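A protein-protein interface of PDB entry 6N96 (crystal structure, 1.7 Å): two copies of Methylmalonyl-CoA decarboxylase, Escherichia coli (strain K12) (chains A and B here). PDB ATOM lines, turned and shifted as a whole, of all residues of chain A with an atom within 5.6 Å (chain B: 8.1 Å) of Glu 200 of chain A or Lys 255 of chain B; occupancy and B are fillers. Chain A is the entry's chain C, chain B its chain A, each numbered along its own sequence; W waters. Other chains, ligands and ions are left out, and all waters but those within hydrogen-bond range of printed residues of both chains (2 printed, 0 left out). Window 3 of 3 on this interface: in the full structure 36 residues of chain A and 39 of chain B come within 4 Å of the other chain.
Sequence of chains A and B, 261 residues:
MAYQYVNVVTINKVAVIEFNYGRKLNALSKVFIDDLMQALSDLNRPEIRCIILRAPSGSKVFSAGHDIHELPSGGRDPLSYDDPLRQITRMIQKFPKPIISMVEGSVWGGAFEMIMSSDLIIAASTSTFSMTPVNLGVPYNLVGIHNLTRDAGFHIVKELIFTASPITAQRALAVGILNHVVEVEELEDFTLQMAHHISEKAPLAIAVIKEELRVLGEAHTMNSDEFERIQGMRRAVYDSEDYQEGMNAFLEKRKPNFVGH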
ATOM      1  N   ARG A  49      -3.251  31.350 -24.933  1.00  0.00           N
ATOM      2  CA  ARG A  49      -2.540  30.960 -26.179  1.00  0.00           C
ATOM      3  C   ARG A  49      -3.394  31.162 -27.436  1.00  0.00           C
ATOM      4  O   ARG A  49      -2.818  31.148 -28.530  1.00  0.00           O
ATOM      5  CB  ARG A  49      -2.118  29.497 -26.122  1.00  0.00           C
ATOM      6  CG  ARG A  49      -1.117  29.197 -25.015  1.00  0.00           C
ATOM      7  CD  ARG A  49       0.124  30.070 -25.019  1.00  0.00           C
ATOM      8  NE  ARG A  49       1.006  29.594 -23.961  1.00  0.00           N
ATOM      9  CZ  ARG A  49       1.706  28.481 -24.006  1.00  0.00           C
ATOM     10  NH1 ARG A  49       1.734  27.757 -25.106  1.00  0.00           N
ATOM     11  NH2 ARG A  49       2.429  28.117 -22.963  1.00  0.00           N
ATOM     12  N   ALA A 195      -8.748  25.478 -31.339  1.00  0.00           N
ATOM     13  CA  ALA A 195      -8.124  26.466 -30.434  1.00  0.00           C
ATOM     14  C   ALA A 195      -7.253  25.736 -29.408  1.00  0.00           C
ATOM     15  O   ALA A 195      -6.138  26.156 -29.107  1.00  0.00           O
ATOM     16  CB  ALA A 195      -9.136  27.349 -29.768  1.00  0.00           C
ATOM     17  N   HIS A 196      -7.745  24.644 -28.857  1.00  0.00           N
ATOM     18  CA  HIS A 196      -6.952  23.861 -27.876  1.00  0.00           C
ATOM     19  C   HIS A 196      -5.717  23.239 -28.542  1.00  0.00           C
ATOM     20  O   HIS A 196      -4.701  23.181 -27.861  1.00  0.00           O
ATOM     21  CB  HIS A 196      -7.832  22.812 -27.205  1.00  0.00           C
ATOM     22  CG  HIS A 196      -8.818  23.371 -26.230  1.00  0.00           C
ATOM     23  ND1 HIS A 196      -8.436  24.034 -25.087  1.00  0.00           N
ATOM     24  CD2 HIS A 196     -10.167  23.300 -26.201  1.00  0.00           C
ATOM     25  CE1 HIS A 196      -9.510  24.395 -24.423  1.00  0.00           C
ATOM     26  NE2 HIS A 196     -10.591  23.918 -25.072  1.00  0.00           N
ATOM     27  N   HIS A 197      -5.853  22.754 -29.767  1.00  0.00           N
ATOM     28  CA  HIS A 197      -4.740  22.173 -30.576  1.00  0.00           C
ATOM     29  C   HIS A 197      -3.664  23.250 -30.786  1.00  0.00           C
ATOM     30  O   HIS A 197      -2.487  23.017 -30.478  1.00  0.00           O
ATOM     31  CB  HIS A 197      -5.255  21.583 -31.892  1.00  0.00           C
ATOM     32  CG  HIS A 197      -4.223  20.765 -32.568  1.00  0.00           C
ATOM     33  ND1 HIS A 197      -3.709  21.095 -33.800  1.00  0.00           N
ATOM     34  CD2 HIS A 197      -3.504  19.722 -32.137  1.00  0.00           C
ATOM     35  CE1 HIS A 197      -2.776  20.225 -34.140  1.00  0.00           C
ATOM     36  NE2 HIS A 197      -2.604  19.390 -33.146  1.00  0.00           N
ATOM     37  N   ILE A 198      -4.073  24.442 -31.216  1.00  0.00           N
ATOM     38  CA  ILE A 198      -3.151  25.602 -31.418  1.00  0.00           C
ATOM     39  C   ILE A 198      -2.443  25.929 -30.109  1.00  0.00           C
ATOM     40  O   ILE A 198      -1.244  26.278 -30.124  1.00  0.00           O
ATOM     41  CB  ILE A 198      -3.904  26.819 -31.968  1.00  0.00           C
ATOM     42  CG1 ILE A 198      -4.338  26.571 -33.409  1.00  0.00           C
ATOM     43  CG2 ILE A 198      -3.057  28.053 -31.821  1.00  0.00           C
ATOM     44  CD1 ILE A 198      -5.276  27.628 -33.917  1.00  0.00           C
ATOM     45  N   SER A 199      -3.150  25.832 -28.995  1.00  0.00           N
ATOM     46  CA  SER A 199      -2.648  26.191 -27.658  1.00  0.00           C
ATOM     47  C   SER A 199      -1.539  25.229 -27.190  1.00  0.00           C
ATOM     48  O   SER A 199      -0.849  25.589 -26.229  1.00  0.00           O
ATOM     49  CB  SER A 199      -3.776  26.318 -26.700  1.00  0.00           C
ATOM     50  OG  SER A 199      -4.560  27.442 -27.132  1.00  0.00           O
ATOM     51  N   GLU A 200      -1.340  24.098 -27.856  1.00  0.00           N
ATOM     52  CA  GLU A 200      -0.208  23.175 -27.568  1.00  0.00           C
ATOM     53  C   GLU A 200       1.085  23.567 -28.298  1.00  0.00           C
ATOM     54  O   GLU A 200       2.135  22.950 -27.996  1.00  0.00           O
ATOM     55  CB  GLU A 200      -0.546  21.764 -28.025  1.00  0.00           C
ATOM     56  CG  GLU A 200      -1.718  21.225 -27.201  1.00  0.00           C
ATOM     57  CD  GLU A 200      -2.262  19.891 -27.715  1.00  0.00           C
ATOM     58  OE1 GLU A 200      -3.198  19.372 -27.059  1.00  0.00           O
ATOM     59  OE2 GLU A 200      -1.738  19.352 -28.753  1.00  0.00           O
ATOM     60  N   LYS A 201       1.014  24.522 -29.212  1.00  0.00           N
ATOM     61  CA  LYS A 201       2.121  24.796 -30.154  1.00  0.00           C
ATOM     62  C   LYS A 201       2.979  25.903 -29.576  1.00  0.00           C
ATOM     63  O   LYS A 201       2.661  26.458 -28.527  1.00  0.00           O
ATOM     64  CB  LYS A 201       1.566  25.073 -31.568  1.00  0.00           C
ATOM     65  CG  LYS A 201       0.633  24.014 -32.107  1.00  0.00           C
ATOM     66  CD  LYS A 201       1.227  22.635 -32.187  1.00  0.00           C
ATOM     67  CE  LYS A 201       0.324  21.615 -32.835  1.00  0.00           C
ATOM     68  NZ  LYS A 201       1.023  20.330 -32.993  1.00  0.00           N
ATOM     69  N   ALA A 202       4.068  26.236 -30.253  1.00  0.00           N
ATOM     70  CA  ALA A 202       5.052  27.186 -29.708  1.00  0.00           C
ATOM     71  C   ALA A 202       4.553  28.621 -29.868  1.00  0.00           C
ATOM     72  O   ALA A 202       4.551  29.168 -30.962  1.00  0.00           O
ATOM     73  CB  ALA A 202       6.342  27.001 -30.429  1.00  0.00           C
ATOM     74  N   VAL B 134       5.733  25.587 -35.836  1.00  0.00           N
ATOM     75  CA  VAL B 134       5.176  25.824 -34.482  1.00  0.00           C
ATOM     76  C   VAL B 134       5.268  24.541 -33.661  1.00  0.00           C
ATOM     77  O   VAL B 134       5.081  24.595 -32.430  1.00  0.00           O
ATOM     78  CB  VAL B 134       3.752  26.389 -34.481  1.00  0.00           C
ATOM     79  CG1 VAL B 134       3.684  27.647 -35.301  1.00  0.00           C
ATOM     80  CG2 VAL B 134       2.677  25.411 -34.896  1.00  0.00           C
ATOM     81  N   ASN B 135       5.554  23.418 -34.296  1.00  0.00           N
ATOM     82  CA  ASN B 135       5.825  22.167 -33.542  1.00  0.00           C
ATOM     83  C   ASN B 135       7.202  22.198 -32.883  1.00  0.00           C
ATOM     84  O   ASN B 135       7.381  21.411 -31.941  1.00  0.00           O
ATOM     85  CB  ASN B 135       5.772  20.949 -34.452  1.00  0.00           C
ATOM     86  CG  ASN B 135       4.382  20.521 -34.822  1.00  0.00           C
ATOM     87  OD1 ASN B 135       3.401  20.989 -34.236  1.00  0.00           O
ATOM     88  ND2 ASN B 135       4.294  19.602 -35.789  1.00  0.00           N
ATOM     89  N   PHE B 162      -0.574  27.679 -37.932  1.00  0.00           N
ATOM     90  CA  PHE B 162      -0.830  27.736 -36.466  1.00  0.00           C
ATOM     91  C   PHE B 162      -1.211  26.368 -35.910  1.00  0.00           C
ATOM     92  O   PHE B 162      -0.946  26.173 -34.729  1.00  0.00           O
ATOM     93  CB  PHE B 162      -1.861  28.800 -36.127  1.00  0.00           C
ATOM     94  CG  PHE B 162      -1.474  30.217 -36.447  1.00  0.00           C
ATOM     95  CD1 PHE B 162      -0.180  30.578 -36.776  1.00  0.00           C
ATOM     96  CD2 PHE B 162      -2.459  31.193 -36.479  1.00  0.00           C
ATOM     97  CE1 PHE B 162       0.152  31.883 -37.106  1.00  0.00           C
ATOM     98  CE2 PHE B 162      -2.123  32.504 -36.797  1.00  0.00           C
ATOM     99  CZ  PHE B 162      -0.825  32.836 -37.131  1.00  0.00           C
ATOM    100  N   THR B 163      -1.834  25.487 -36.681  1.00  0.00           N
ATOM    101  CA  THR B 163      -2.282  24.157 -36.219  1.00  0.00           C
ATOM    102  C   THR B 163      -1.189  23.141 -36.462  1.00  0.00           C
ATOM    103  O   THR B 163      -1.158  22.138 -35.760  1.00  0.00           O
ATOM    104  CB  THR B 163      -3.552  23.655 -36.917  1.00  0.00           C
ATOM    105  OG1 THR B 163      -3.357  23.451 -38.321  1.00  0.00           O
ATOM    106  CG2 THR B 163      -4.720  24.585 -36.722  1.00  0.00           C
ATOM    107  N   GLU B 245      13.554  23.710 -26.219  1.00  0.00           N
ATOM    108  CA  GLU B 245      12.569  22.651 -25.838  1.00  0.00           C
ATOM    109  C   GLU B 245      12.107  21.967 -27.123  1.00  0.00           C
ATOM    110  O   GLU B 245      11.939  20.729 -27.119  1.00  0.00           O
ATOM    111  CB  GLU B 245      11.406  23.264 -25.067  1.00  0.00           C
ATOM    112  CG  GLU B 245      10.233  22.343 -24.855  1.00  0.00           C
ATOM    113  CD  GLU B 245      10.497  21.128 -23.952  1.00  0.00           C
ATOM    114  OE1 GLU B 245      11.666  20.938 -23.509  1.00  0.00           O
ATOM    115  OE2 GLU B 245       9.549  20.345 -23.739  1.00  0.00           O
ATOM    116  N   GLY B 246      11.809  22.717 -28.186  1.00  0.00           N
ATOM    117  CA  GLY B 246      11.288  22.151 -29.441  1.00  0.00           C
ATOM    118  C   GLY B 246      12.334  21.225 -30.047  1.00  0.00           C
ATOM    119  O   GLY B 246      11.970  20.105 -30.481  1.00  0.00           O
ATOM    120  N   ASN B 248      14.856  19.711 -28.345  1.00  0.00           N
ATOM    121  CA  ASN B 248      15.087  18.618 -27.360  1.00  0.00           C
ATOM    122  C   ASN B 248      13.950  17.594 -27.483  1.00  0.00           C
ATOM    123  O   ASN B 248      14.235  16.369 -27.494  1.00  0.00           O
ATOM    124  CB  ASN B 248      15.252  19.184 -25.940  1.00  0.00           C
ATOM    125  CG  ASN B 248      16.573  19.898 -25.727  1.00  0.00           C
ATOM    126  OD1 ASN B 248      16.768  20.585 -24.723  1.00  0.00           O
ATOM    127  ND2 ASN B 248      17.505  19.710 -26.646  1.00  0.00           N
ATOM    128  N   ALA B 249      12.696  18.061 -27.559  1.00  0.00           N
ATOM    129  CA  ALA B 249      11.527  17.177 -27.627  1.00  0.00           C
ATOM    130  C   ALA B 249      11.659  16.293 -28.863  1.00  0.00           C
ATOM    131  O   ALA B 249      11.325  15.099 -28.828  1.00  0.00           O
ATOM    132  CB  ALA B 249      10.242  17.956 -27.643  1.00  0.00           C
ATOM    133  N   PHE B 250      12.092  16.852 -29.985  1.00  0.00           N
ATOM    134  CA  PHE B 250      12.202  16.037 -31.210  1.00  0.00           C
ATOM    135  C   PHE B 250      13.280  14.964 -30.971  1.00  0.00           C
ATOM    136  O   PHE B 250      13.038  13.821 -31.340  1.00  0.00           O
ATOM    137  CB  PHE B 250      12.513  16.893 -32.443  1.00  0.00           C
ATOM    138  CG  PHE B 250      12.675  16.031 -33.656  1.00  0.00           C
ATOM    139  CD1 PHE B 250      11.556  15.497 -34.254  1.00  0.00           C
ATOM    140  CD2 PHE B 250      13.927  15.639 -34.094  1.00  0.00           C
ATOM    141  CE1 PHE B 250      11.675  14.642 -35.337  1.00  0.00           C
ATOM    142  CE2 PHE B 250      14.043  14.775 -35.179  1.00  0.00           C
ATOM    143  CZ  PHE B 250      12.920  14.274 -35.782  1.00  0.00           C
ATOM    144  N   GLU B 252      14.362  13.672 -28.261  1.00  0.00           N
ATOM    145  CA  GLU B 252      13.926  12.724 -27.200  1.00  0.00           C
ATOM    146  C   GLU B 252      12.622  12.018 -27.563  1.00  0.00           C
ATOM    147  O   GLU B 252      12.179  11.194 -26.765  1.00  0.00           O
ATOM    148  CB  GLU B 252      13.816  13.467 -25.870  1.00  0.00           C
ATOM    149  CG  GLU B 252      15.158  13.950 -25.379  1.00  0.00           C
ATOM    150  CD  GLU B 252      15.162  14.626 -24.021  1.00  0.00           C
ATOM    151  OE1 GLU B 252      14.089  14.695 -23.354  1.00  0.00           O
ATOM    152  OE2 GLU B 252      16.251  15.084 -23.617  1.00  0.00           O
ATOM    153  N   LYS B 253      11.993  12.341 -28.692  1.00  0.00           N
ATOM    154  CA  LYS B 253      10.813  11.603 -29.185  1.00  0.00           C
ATOM    155  C   LYS B 253       9.689  11.753 -28.158  1.00  0.00           C
ATOM    156  O   LYS B 253       9.040  10.742 -27.821  1.00  0.00           O
ATOM    157  CB  LYS B 253      11.174  10.135 -29.477  1.00  0.00           C
ATOM    158  CG  LYS B 253      12.210   9.918 -30.580  1.00  0.00           C
ATOM    159  CD  LYS B 253      12.202   8.484 -31.132  1.00  0.00           C
ATOM    160  CE  LYS B 253      13.510   8.034 -31.756  1.00  0.00           C
ATOM    161  NZ  LYS B 253      13.990   8.956 -32.822  1.00  0.00           N
ATOM    162  N   ARG B 254       9.438  12.993 -27.718  1.00  0.00           N
ATOM    163  CA  ARG B 254       8.378  13.325 -26.737  1.00  0.00           C
ATOM    164  C   ARG B 254       7.660  14.600 -27.200  1.00  0.00           C
ATOM    165  O   ARG B 254       8.136  15.279 -28.159  1.00  0.00           O
ATOM    166  CB  ARG B 254       8.911  13.482 -25.306  1.00  0.00           C
ATOM    167  CG  ARG B 254      10.018  14.509 -25.161  1.00  0.00           C
ATOM    168  CD  ARG B 254      10.478  14.753 -23.754  1.00  0.00           C
ATOM    169  NE  ARG B 254      11.471  15.787 -23.782  1.00  0.00           N
ATOM    170  CZ  ARG B 254      11.228  17.084 -23.738  1.00  0.00           C
ATOM    171  NH1 ARG B 254       9.982  17.539 -23.723  1.00  0.00           N
ATOM    172  NH2 ARG B 254      12.253  17.923 -23.787  1.00  0.00           N
ATOM    173  N   LYS B 255       6.534  14.874 -26.559  1.00  0.00           N
ATOM    174  CA  LYS B 255       5.730  16.081 -26.862  1.00  0.00           C
ATOM    175  C   LYS B 255       6.345  17.279 -26.145  1.00  0.00           C
ATOM    176  O   LYS B 255       6.607  17.256 -24.934  1.00  0.00           O
ATOM    177  CB  LYS B 255       4.298  15.769 -26.446  1.00  0.00           C
ATOM    178  CG  LYS B 255       3.290  16.895 -26.485  1.00  0.00           C
ATOM    179  CD  LYS B 255       1.932  16.382 -25.981  1.00  0.00           C
ATOM    180  CE  LYS B 255       0.762  17.115 -26.593  1.00  0.00           C
ATOM    181  NZ  LYS B 255       0.776  18.518 -26.127  1.00  0.00           N
ATOM    182  N   PRO B 256       6.627  18.380 -26.866  1.00  0.00           N
ATOM    183  CA  PRO B 256       7.221  19.536 -26.230  1.00  0.00           C
ATOM    184  C   PRO B 256       6.238  20.194 -25.271  1.00  0.00           C
ATOM    185  O   PRO B 256       5.077  20.151 -25.535  1.00  0.00           O
ATOM    186  CB  PRO B 256       7.605  20.474 -27.387  1.00  0.00           C
ATOM    187  CG  PRO B 256       6.681  20.067 -28.512  1.00  0.00           C
ATOM    188  CD  PRO B 256       6.415  18.578 -28.310  1.00  0.00           C
ATOM    189  N   ASN B 257       6.771  20.760 -24.201  1.00  0.00           N
ATOM    190  CA  ASN B 257       6.039  21.623 -23.249  1.00  0.00           C
ATOM    191  C   ASN B 257       6.471  23.072 -23.477  1.00  0.00           C
ATOM    192  O   ASN B 257       7.412  23.513 -22.861  1.00  0.00           O
ATOM    193  CB  ASN B 257       6.287  21.248 -21.783  1.00  0.00           C
ATOM    194  CG  ASN B 257       5.391  22.063 -20.874  1.00  0.00           C
ATOM    195  OD1 ASN B 257       4.216  22.252 -21.178  1.00  0.00           O
ATOM    196  ND2 ASN B 257       5.938  22.629 -19.810  1.00  0.00           N
ATOM    197  N   PHE B 258       5.755  23.825 -24.313  1.00  0.00           N
ATOM    198  CA  PHE B 258       6.137  25.233 -24.541  1.00  0.00           C
ATOM    199  C   PHE B 258       5.462  26.128 -23.489  1.00  0.00           C
ATOM    200  O   PHE B 258       4.253  25.915 -23.167  1.00  0.00           O
ATOM    201  CB  PHE B 258       5.721  25.640 -25.942  1.00  0.00           C
ATOM    202  CG  PHE B 258       6.338  24.874 -27.067  1.00  0.00           C
ATOM    203  CD1 PHE B 258       7.698  24.929 -27.256  1.00  0.00           C
ATOM    204  CD2 PHE B 258       5.556  24.091 -27.925  1.00  0.00           C
ATOM    205  CE1 PHE B 258       8.283  24.281 -28.320  1.00  0.00           C
ATOM    206  CE2 PHE B 258       6.147  23.439 -28.989  1.00  0.00           C
ATOM    207  CZ  PHE B 258       7.515  23.540 -29.192  1.00  0.00           C
ATOM    208  N   VAL B 259       6.179  27.150 -23.060  1.00  0.00           N
ATOM    209  CA  VAL B 259       5.766  28.062 -21.953  1.00  0.00           C
ATOM    210  C   VAL B 259       5.776  29.541 -22.365  1.00  0.00           C
ATOM    211  O   VAL B 259       5.335  30.360 -21.575  1.00  0.00           O
ATOM    212  CB  VAL B 259       6.654  27.818 -20.717  1.00  0.00           C
ATOM    213  CG1 VAL B 259       6.481  26.390 -20.209  1.00  0.00           C
ATOM    214  CG2 VAL B 259       8.121  28.157 -20.977  1.00  0.00           C
HETATM  215  O   HOH W   1      -0.302  19.225 -35.387  1.00  0.00           O
HETATM  216  O   HOH W   2       3.043  23.118 -25.200  1.00  0.00           O
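O of Val 134 of chain B is in hydrogen-bond range of N of Ala 202 of chain A, 2.9 Å away. The side-chain amide oxygen (OD1) of Asn 135 of chain B is in hydrogen-bond range of the side-chain amino group (NZ) of Lys 201 of chain A. ND1 of His 197 of chain A lies close to O of Thr 163 of chain B, at 3.4 Å. The side-chain amino group (NZ) of Lys 255 of chain B is in salt-bridge range of the side-chain carboxylate (OE2) of Glu 200 of chain A (3.7 Å). The backbone carbonyl oxygen (O) of Phe 258 of chain B lies within hydrogen-bond range of the guanidinium group (NH2) of Arg 49 of chain A (2.9 Å).
CA of Val 259 of chain B touches NH2 of Arg 49 of chain A, at 3.5 Å. CG1 of Ile 198 of chain A touches O of Phe 162 of chain B (3.7 Å). CG1 of Ile 198 of chain A touches CG2 of Thr 163 of chain B (3.9 Å). Phe 258 of chain B touches Glu 200 of chain A (CD2 to O, 3.6 Å). CB of Lys 201 of chain A touches CG2 of Val 134 of chain B (3.5 Å). Lys 201 of chain A touches Phe 162 of chain B (CG to O, 3.7 Å). O of Thr 163 of chain B touches CE of Lys 201 of chain A, 3.3 Å away. Phe 258 of chain B touches Lys 201 of chain A (CD2 to C, 3.6 Å). CD2 of Phe 258 of chain B touches N of Ala 202 of chain A, at 3.5 Å.
Of chain B, only Lys 255 (3.7 Å) and Phe 258 (3.6 Å) come within 4 Å of Glu 200 of chain A. Lys 255 of chain B touches just one residue of chain A: Glu 200. Printed residues of chain A within 4 Å of Asn 135 of chain B: Lys 201. Printed residues of chain B within 4 Å of Ala 202 of chain A: Val 134 (2.9 Å) and Phe 258 (3.5 Å). Of the printed residues of chain B, His 197 of chain A touches Thr 163 (3.0 Å). Of the printed residues of chain A, Thr 163 of chain B touches His 197 (3.0 Å), Ile 198 (3.9 Å) and Lys 201 (3.3 Å). Of the printed residues of chain A, Phe 258 of chain B touches Arg 49, Glu 200, Lys 201 and Ala 202. Phe 250 of chain B touches none of the printed residues of chain A. Ala 249 of chain B touches none of the printed residues of chain A. The nearest printed residue of chain B that does not touch Ile 198 of chain A is Val 134 of chain B (6.2 Å).
Hydrophobic or aromatic side chains of chain B that line the printed part of chain A: Val 134 and Phe 258. Among the printed residues, Asp or Glu carboxylates within 4 Å of a Lys or Arg side-chain nitrogen of the other chain: Glu 200 of chain A with Lys 255 of chain B (3.7 Å).
No position is printed for both chains.
Water W2 lies within hydrogen-bond range of the backbone NH (N) of Phe 258 of chain B and the backbone carbonyl oxygen (O) of Glu 200 of chain A. Water W1 lies within hydrogen-bond range of the side-chain amino group of Lys 201 of chain A, the backbone carbonyl oxygen of Thr 163 of chain B and a ring nitrogen (NE2) of His 197 of chain A.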
